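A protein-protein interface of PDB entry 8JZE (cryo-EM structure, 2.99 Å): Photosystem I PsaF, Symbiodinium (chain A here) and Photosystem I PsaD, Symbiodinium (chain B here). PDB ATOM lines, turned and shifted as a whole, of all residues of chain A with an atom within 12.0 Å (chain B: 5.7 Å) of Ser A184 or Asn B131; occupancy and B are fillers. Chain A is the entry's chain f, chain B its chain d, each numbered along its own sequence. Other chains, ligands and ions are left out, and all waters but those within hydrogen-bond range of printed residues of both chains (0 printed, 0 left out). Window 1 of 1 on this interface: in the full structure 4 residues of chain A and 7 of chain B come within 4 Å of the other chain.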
ATOM      1  N   GLY A 179       9.578   2.611  26.430  1.00  0.00           N
ATOM      2  CA  GLY A 179      10.456   1.647  25.816  1.00  0.00           C
ATOM      3  C   GLY A 179      10.839   0.530  26.761  1.00  0.00           C
ATOM      4  O   GLY A 179      10.985   0.727  27.972  1.00  0.00           O
ATOM      5  N   PRO A 180      10.999  -0.677  26.222  1.00  0.00           N
ATOM      6  CA  PRO A 180      11.455  -1.794  27.052  1.00  0.00           C
ATOM      7  C   PRO A 180      12.877  -1.570  27.535  1.00  0.00           C
ATOM      8  O   PRO A 180      13.741  -1.101  26.791  1.00  0.00           O
ATOM      9  CB  PRO A 180      11.366  -2.999  26.108  1.00  0.00           C
ATOM     10  CG  PRO A 180      11.501  -2.412  24.748  1.00  0.00           C
ATOM     11  CD  PRO A 180      10.821  -1.071  24.816  1.00  0.00           C
ATOM     12  N   TRP A 181      13.136  -1.957  28.778  1.00  0.00           N
ATOM     13  CA  TRP A 181      14.458  -1.790  29.343  1.00  0.00           C
ATOM     14  C   TRP A 181      15.098  -3.110  29.663  1.00  0.00           C
ATOM     15  O   TRP A 181      16.179  -3.125  30.224  1.00  0.00           O
ATOM     16  CB  TRP A 181      14.364  -0.970  30.612  1.00  0.00           C
ATOM     17  CG  TRP A 181      13.508  -1.548  31.701  1.00  0.00           C
ATOM     18  CD1 TRP A 181      13.909  -2.377  32.704  1.00  0.00           C
ATOM     19  CD2 TRP A 181      12.117  -1.305  31.920  1.00  0.00           C
ATOM     20  NE1 TRP A 181      12.852  -2.688  33.513  1.00  0.00           N
ATOM     21  CE2 TRP A 181      11.740  -2.038  33.057  1.00  0.00           C
ATOM     22  CE3 TRP A 181      11.151  -0.546  31.257  1.00  0.00           C
ATOM     23  CZ2 TRP A 181      10.444  -2.036  33.547  1.00  0.00           C
ATOM     24  CZ3 TRP A 181       9.865  -0.545  31.743  1.00  0.00           C
ATOM     25  CH2 TRP A 181       9.521  -1.285  32.877  1.00  0.00           C
ATOM     26  N   ASN A 182      14.411  -4.199  29.322  1.00  0.00           N
ATOM     27  CA  ASN A 182      14.880  -5.531  29.651  1.00  0.00           C
ATOM     28  C   ASN A 182      14.106  -6.619  28.989  1.00  0.00           C
ATOM     29  O   ASN A 182      12.963  -6.380  28.619  1.00  0.00           O
ATOM     30  CB  ASN A 182      14.702  -5.798  31.140  1.00  0.00           C
ATOM     31  CG  ASN A 182      13.297  -5.467  31.663  1.00  0.00           C
ATOM     32  OD1 ASN A 182      12.451  -4.897  30.977  1.00  0.00           O
ATOM     33  ND2 ASN A 182      13.063  -5.804  32.916  1.00  0.00           N
ATOM     34  N   GLN A 183      14.702  -7.792  28.812  1.00  0.00           N
ATOM     35  CA  GLN A 183      14.007  -8.982  28.329  1.00  0.00           C
ATOM     36  C   GLN A 183      14.929 -10.191  28.419  1.00  0.00           C
ATOM     37  O   GLN A 183      14.674 -11.116  29.197  1.00  0.00           O
ATOM     38  CB  GLN A 183      13.521  -8.810  26.889  1.00  0.00           C
ATOM     39  CG  GLN A 183      12.109  -9.331  26.642  1.00  0.00           C
ATOM     40  CD  GLN A 183      12.000 -10.840  26.753  1.00  0.00           C
ATOM     41  OE1 GLN A 183      12.985 -11.560  26.597  1.00  0.00           O
ATOM     42  NE2 GLN A 183      10.794 -11.327  27.023  1.00  0.00           N
ATOM     43  N   SER A 184      16.002 -10.180  27.633  1.00  0.00           N
ATOM     44  CA  SER A 184      16.947 -11.291  27.549  1.00  0.00           C
ATOM     45  C   SER A 184      16.246 -12.609  27.232  1.00  0.00           C
ATOM     46  O   SER A 184      16.845 -13.678  27.341  1.00  0.00           O
ATOM     47  CB  SER A 184      17.750 -11.425  28.847  1.00  0.00           C
ATOM     48  OG  SER A 184      16.934 -11.862  29.919  1.00  0.00           O
ATOM     49  N   ARG B 124      17.710 -15.182  13.754  1.00  0.00           N
ATOM     50  CA  ARG B 124      17.586 -15.260  15.204  1.00  0.00           C
ATOM     51  C   ARG B 124      16.170 -15.689  15.563  1.00  0.00           C
ATOM     52  O   ARG B 124      15.204 -15.011  15.171  1.00  0.00           O
ATOM     53  CB  ARG B 124      17.935 -13.917  15.852  1.00  0.00           C
ATOM     54  CG  ARG B 124      19.314 -13.400  15.461  1.00  0.00           C
ATOM     55  CD  ARG B 124      19.797 -12.280  16.366  1.00  0.00           C
ATOM     56  NE  ARG B 124      19.891 -12.699  17.759  1.00  0.00           N
ATOM     57  CZ  ARG B 124      20.896 -13.397  18.268  1.00  0.00           C
ATOM     58  NH1 ARG B 124      21.911 -13.794  17.518  1.00  0.00           N
ATOM     59  NH2 ARG B 124      20.883 -13.705  19.561  1.00  0.00           N
ATOM     60  N   PHE B 126      13.667 -15.475  17.607  1.00  0.00           N
ATOM     61  CA  PHE B 126      12.837 -14.782  18.586  1.00  0.00           C
ATOM     62  C   PHE B 126      12.597 -13.364  18.089  1.00  0.00           C
ATOM     63  O   PHE B 126      13.196 -12.921  17.107  1.00  0.00           O
ATOM     64  CB  PHE B 126      13.470 -14.769  19.982  1.00  0.00           C
ATOM     65  CG  PHE B 126      14.963 -14.606  19.978  1.00  0.00           C
ATOM     66  CD1 PHE B 126      15.545 -13.394  19.649  1.00  0.00           C
ATOM     67  CD2 PHE B 126      15.784 -15.664  20.327  1.00  0.00           C
ATOM     68  CE1 PHE B 126      16.916 -13.244  19.653  1.00  0.00           C
ATOM     69  CE2 PHE B 126      17.154 -15.523  20.336  1.00  0.00           C
ATOM     70  CZ  PHE B 126      17.721 -14.311  19.998  1.00  0.00           C
ATOM     71  N   THR B 127      11.704 -12.659  18.782  1.00  0.00           N
ATOM     72  CA  THR B 127      11.508 -11.245  18.510  1.00  0.00           C
ATOM     73  C   THR B 127      12.792 -10.480  18.812  1.00  0.00           C
ATOM     74  O   THR B 127      13.656 -10.937  19.561  1.00  0.00           O
ATOM     75  CB  THR B 127      10.357 -10.683  19.343  1.00  0.00           C
ATOM     76  OG1 THR B 127      10.687 -10.767  20.734  1.00  0.00           O
ATOM     77  CG2 THR B 127       9.084 -11.465  19.090  1.00  0.00           C
ATOM     78  N   ILE B 128      12.909  -9.293  18.213  1.00  0.00           N
ATOM     79  CA  ILE B 128      14.127  -8.503  18.365  1.00  0.00           C
ATOM     80  C   ILE B 128      14.384  -8.177  19.829  1.00  0.00           C
ATOM     81  O   ILE B 128      15.539  -8.051  20.255  1.00  0.00           O
ATOM     82  CB  ILE B 128      14.039  -7.232  17.497  1.00  0.00           C
ATOM     83  CG1 ILE B 128      15.275  -6.346  17.688  1.00  0.00           C
ATOM     84  CG2 ILE B 128      12.762  -6.478  17.802  1.00  0.00           C
ATOM     85  CD1 ILE B 128      15.365  -5.204  16.698  1.00  0.00           C
ATOM     86  N   ARG B 129      13.324  -8.060  20.630  1.00  0.00           N
ATOM     87  CA  ARG B 129      13.495  -7.801  22.053  1.00  0.00           C
ATOM     88  C   ARG B 129      14.037  -9.008  22.810  1.00  0.00           C
ATOM     89  O   ARG B 129      14.512  -8.846  23.937  1.00  0.00           O
ATOM     90  CB  ARG B 129      12.166  -7.341  22.664  1.00  0.00           C
ATOM     91  CG  ARG B 129      12.231  -6.806  24.101  1.00  0.00           C
ATOM     92  CD  ARG B 129      13.280  -5.717  24.280  1.00  0.00           C
ATOM     93  NE  ARG B 129      14.618  -6.273  24.441  1.00  0.00           N
ATOM     94  CZ  ARG B 129      15.741  -5.586  24.299  1.00  0.00           C
ATOM     95  NH1 ARG B 129      15.730  -4.288  24.050  1.00  0.00           N
ATOM     96  NH2 ARG B 129      16.904  -6.221  24.398  1.00  0.00           N
ATOM     97  N   GLY B 130      14.015 -10.197  22.212  1.00  0.00           N
ATOM     98  CA  GLY B 130      14.491 -11.389  22.886  1.00  0.00           C
ATOM     99  C   GLY B 130      15.990 -11.479  23.064  1.00  0.00           C
ATOM    100  O   GLY B 130      16.461 -12.425  23.701  1.00  0.00           O
ATOM    101  N   ASN B 131      16.749 -10.530  22.521  1.00  0.00           N
ATOM    102  CA  ASN B 131      18.196 -10.564  22.646  1.00  0.00           C
ATOM    103  C   ASN B 131      18.617 -10.405  24.107  1.00  0.00           C
ATOM    104  O   ASN B 131      17.975  -9.680  24.872  1.00  0.00           O
ATOM    105  CB  ASN B 131      18.832  -9.460  21.804  1.00  0.00           C
ATOM    106  CG  ASN B 131      18.788  -9.761  20.321  1.00  0.00           C
ATOM    107  OD1 ASN B 131      19.022 -10.892  19.900  1.00  0.00           O
ATOM    108  ND2 ASN B 131      18.482  -8.748  19.521  1.00  0.00           N
ATOM    109  N   PRO B 132      19.694 -11.070  24.516  1.00  0.00           N
ATOM    110  CA  PRO B 132      20.149 -10.960  25.904  1.00  0.00           C
ATOM    111  C   PRO B 132      20.697  -9.575  26.206  1.00  0.00           C
ATOM    112  O   PRO B 132      21.152  -8.845  25.322  1.00  0.00           O
ATOM    113  CB  PRO B 132      21.248 -12.022  26.001  1.00  0.00           C
ATOM    114  CG  PRO B 132      21.773 -12.130  24.619  1.00  0.00           C
ATOM    115  CD  PRO B 132      20.590 -11.917  23.710  1.00  0.00           C
ATOM    116  N   GLN B 133      20.643  -9.216  27.485  1.00  0.00           N
ATOM    117  CA  GLN B 133      21.176  -7.936  27.924  1.00  0.00           C
ATOM    118  C   GLN B 133      22.689  -7.904  27.747  1.00  0.00           C
ATOM    119  O   GLN B 133      23.378  -8.903  27.974  1.00  0.00           O
ATOM    120  CB  GLN B 133      20.815  -7.684  29.388  1.00  0.00           C
ATOM    121  CG  GLN B 133      19.369  -8.001  29.740  1.00  0.00           C
ATOM    122  CD  GLN B 133      19.052  -7.741  31.201  1.00  0.00           C
ATOM    123  OE1 GLN B 133      19.871  -7.195  31.939  1.00  0.00           O
ATOM    124  NE2 GLN B 133      17.857  -8.133  31.627  1.00  0.00           N
ATOM    125  N   GLY B 146      25.809  -8.389  22.335  1.00  0.00           N
ATOM    126  CA  GLY B 146      24.694  -9.189  22.815  1.00  0.00           C
ATOM    127  C   GLY B 146      23.753  -9.672  21.730  1.00  0.00           C
ATOM    128  O   GLY B 146      23.047 -10.666  21.932  1.00  0.00           O
ATOM    129  N   TYR B 147      23.722  -8.995  20.582  1.00  0.00           N
ATOM    130  CA  TYR B 147      22.885  -9.426  19.469  1.00  0.00           C
ATOM    131  C   TYR B 147      23.483 -10.589  18.689  1.00  0.00           C
ATOM    132  O   TYR B 147      22.810 -11.127  17.803  1.00  0.00           O
ATOM    133  CB  TYR B 147      22.622  -8.253  18.520  1.00  0.00           C
ATOM    134  CG  TYR B 147      23.868  -7.560  18.015  1.00  0.00           C
ATOM    135  CD1 TYR B 147      24.530  -8.017  16.883  1.00  0.00           C
ATOM    136  CD2 TYR B 147      24.376  -6.443  18.664  1.00  0.00           C
ATOM    137  CE1 TYR B 147      25.663  -7.386  16.418  1.00  0.00           C
ATOM    138  CE2 TYR B 147      25.508  -5.805  18.205  1.00  0.00           C
ATOM    139  CZ  TYR B 147      26.148  -6.281  17.082  1.00  0.00           C
ATOM    140  OH  TYR B 147      27.278  -5.650  16.620  1.00  0.00           O
ATOM    141  N   THR B 154      21.203 -17.097  25.112  1.00  0.00           N
ATOM    142  CA  THR B 154      20.143 -16.173  25.500  1.00  0.00           C
ATOM    143  C   THR B 154      19.205 -16.811  26.515  1.00  0.00           C
ATOM    144  O   THR B 154      18.843 -16.185  27.517  1.00  0.00           O
ATOM    145  CB  THR B 154      19.359 -15.717  24.271  1.00  0.00           C
ATOM    146  OG1 THR B 154      18.467 -16.759  23.861  1.00  0.00           O
ATOM    147  CG2 THR B 154      20.302 -15.401  23.129  1.00  0.00           C
ATOM    148  N   MET B 155      18.812 -18.065  26.281  1.00  0.00           N
ATOM    149  CA  MET B 155      17.966 -18.758  27.249  1.00  0.00           C
ATOM    150  C   MET B 155      18.691 -18.965  28.572  1.00  0.00           C
ATOM    151  O   MET B 155      18.084 -18.864  29.642  1.00  0.00           O
ATOM    152  CB  MET B 155      17.501 -20.100  26.690  1.00  0.00           C
ATOM    153  CG  MET B 155      16.415 -20.015  25.642  1.00  0.00           C
ATOM    154  SD  MET B 155      15.876 -21.671  25.186  1.00  0.00           S
ATOM    155  CE  MET B 155      17.456 -22.502  25.089  1.00  0.00           C
ATOM    156  N   VAL B 157      21.104 -17.099  29.950  1.00  0.00           N
ATOM    157  CA  VAL B 157      21.173 -15.851  30.702  1.00  0.00           C
ATOM    158  C   VAL B 157      19.785 -15.415  31.157  1.00  0.00           C
ATOM    159  O   VAL B 157      19.645 -14.787  32.209  1.00  0.00           O
ATOM    160  CB  VAL B 157      21.883 -14.754  29.886  1.00  0.00           C
ATOM    161  CG1 VAL B 157      23.285 -15.196  29.506  1.00  0.00           C
ATOM    162  CG2 VAL B 157      21.089 -14.389  28.658  1.00  0.00           C
ATOM    163  N   LYS B 158      18.739 -15.741  30.391  1.00  0.00           N
ATOM    164  CA  LYS B 158      17.379 -15.450  30.837  1.00  0.00           C
ATOM    165  C   LYS B 158      17.031 -16.249  32.087  1.00  0.00           C
ATOM    166  O   LYS B 158      16.435 -15.717  33.032  1.00  0.00           O
ATOM    167  CB  LYS B 158      16.392 -15.748  29.710  1.00  0.00           C
ATOM    168  CG  LYS B 158      14.977 -15.253  29.945  1.00  0.00           C
ATOM    169  CD  LYS B 158      14.129 -15.457  28.698  1.00  0.00           C
ATOM    170  CE  LYS B 158      12.716 -14.941  28.893  1.00  0.00           C
ATOM    171  NZ  LYS B 158      11.893 -15.097  27.661  1.00  0.00           N
ATOM    172  N   VAL B 161      18.797 -14.682  34.951  1.00  0.00           N
ATOM    173  CA  VAL B 161      18.078 -13.493  35.400  1.00  0.00           C
ATOM    174  C   VAL B 161      16.883 -13.888  36.255  1.00  0.00           C
ATOM    175  O   VAL B 161      16.612 -13.276  37.296  1.00  0.00           O
ATOM    176  CB  VAL B 161      17.655 -12.636  34.192  1.00  0.00           C
ATOM    177  CG1 VAL B 161      16.651 -11.583  34.614  1.00  0.00           C
ATOM    178  CG2 VAL B 161      18.868 -11.983  33.561  1.00  0.00           C
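The backbone NH (N) of Ser A184 sits close to the backbone carbonyl oxygen (O) of Asn B131, 3.4 Å away.
The backbone carbonyl oxygen (O) of Ser A184 lies close to the backbone carbonyl oxygen (O) of Thr B154 (3.2 Å).
Of chain B, only Gly B130, Asn B131, Pro B132, Gln B133, Thr B154 and Lys B158 come within 4 Å of Ser A184.
Of chain A, only Ser A184 (3.3 Å) comes within 4 Å of Asn B131.
No residue of chain A comes within 4 Å of Arg B124.
No residue of chain A comes within 4 Å of Phe B126.
No residue of chain A comes within 4 Å of Ile B128.
Printed residues of chain A within 4 Å of Arg B129: Pro A180 and Gln A183.
Printed residues of chain A within 4 Å of Pro B132: Ser A184.
Of chain A, only Ser A184 (3.2 Å) comes within 4 Å of Thr B154.
Of chain A, only Gln A183 and Ser A184 come within 4 Å of Lys B158.
Printed residues of chain A within 4 Å of Gly B130: Ser A184.
Printed residues of chain B within 4 Å of Pro A180: Arg B129.
Tyr B147 touches none of the printed residues of chain A.
The nearest residue of chain B that does not touch Ser A184 is Val B161 (4.1 Å).
The nearest printed residue of chain B that does not touch Gln A183 is Gly B130 (4.01 Å).
Among the printed residues, pairs that only touch across the chains: Pro A180 with Arg B129, Asn A182 with Gln B133, Gln A183 with Arg B129, Gln A183 with Lys B158, Ser A184 with Gly B130, Ser A184 with Pro B132, Ser A184 with Gln B133 and Ser A184 with Lys B158.
Of the 6 printed residues of chain A, 4 touch a printed residue of chain B.
Printed residues of chain A that touch a printed residue of chain B: Pro A180, Asn A182, Gln A183 and Ser A184.
Hydrophobic or aromatic side chains of chain A that line the printed part of chain B: Pro A180.
Of the 16 printed residues of chain B, 7 touch a printed residue of chain A.
Among the printed residues, no Asp or Glu carboxylate lies within 4 Å of a Lys or Arg side-chain nitrogen of the other chain.
ND2 of Asn A182 sits close to NE1 of Trp A181, at 3.2 Å.
NE of Arg B124 sits at hydrogen-bond distance from OD1 of Asn B131, 2.9 Å away.
The backbone carbonyl oxygen (O) of Ile B128 is in hydrogen-bond range of the side-chain amide nitrogen (ND2) of Asn B131 (3.1 Å).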
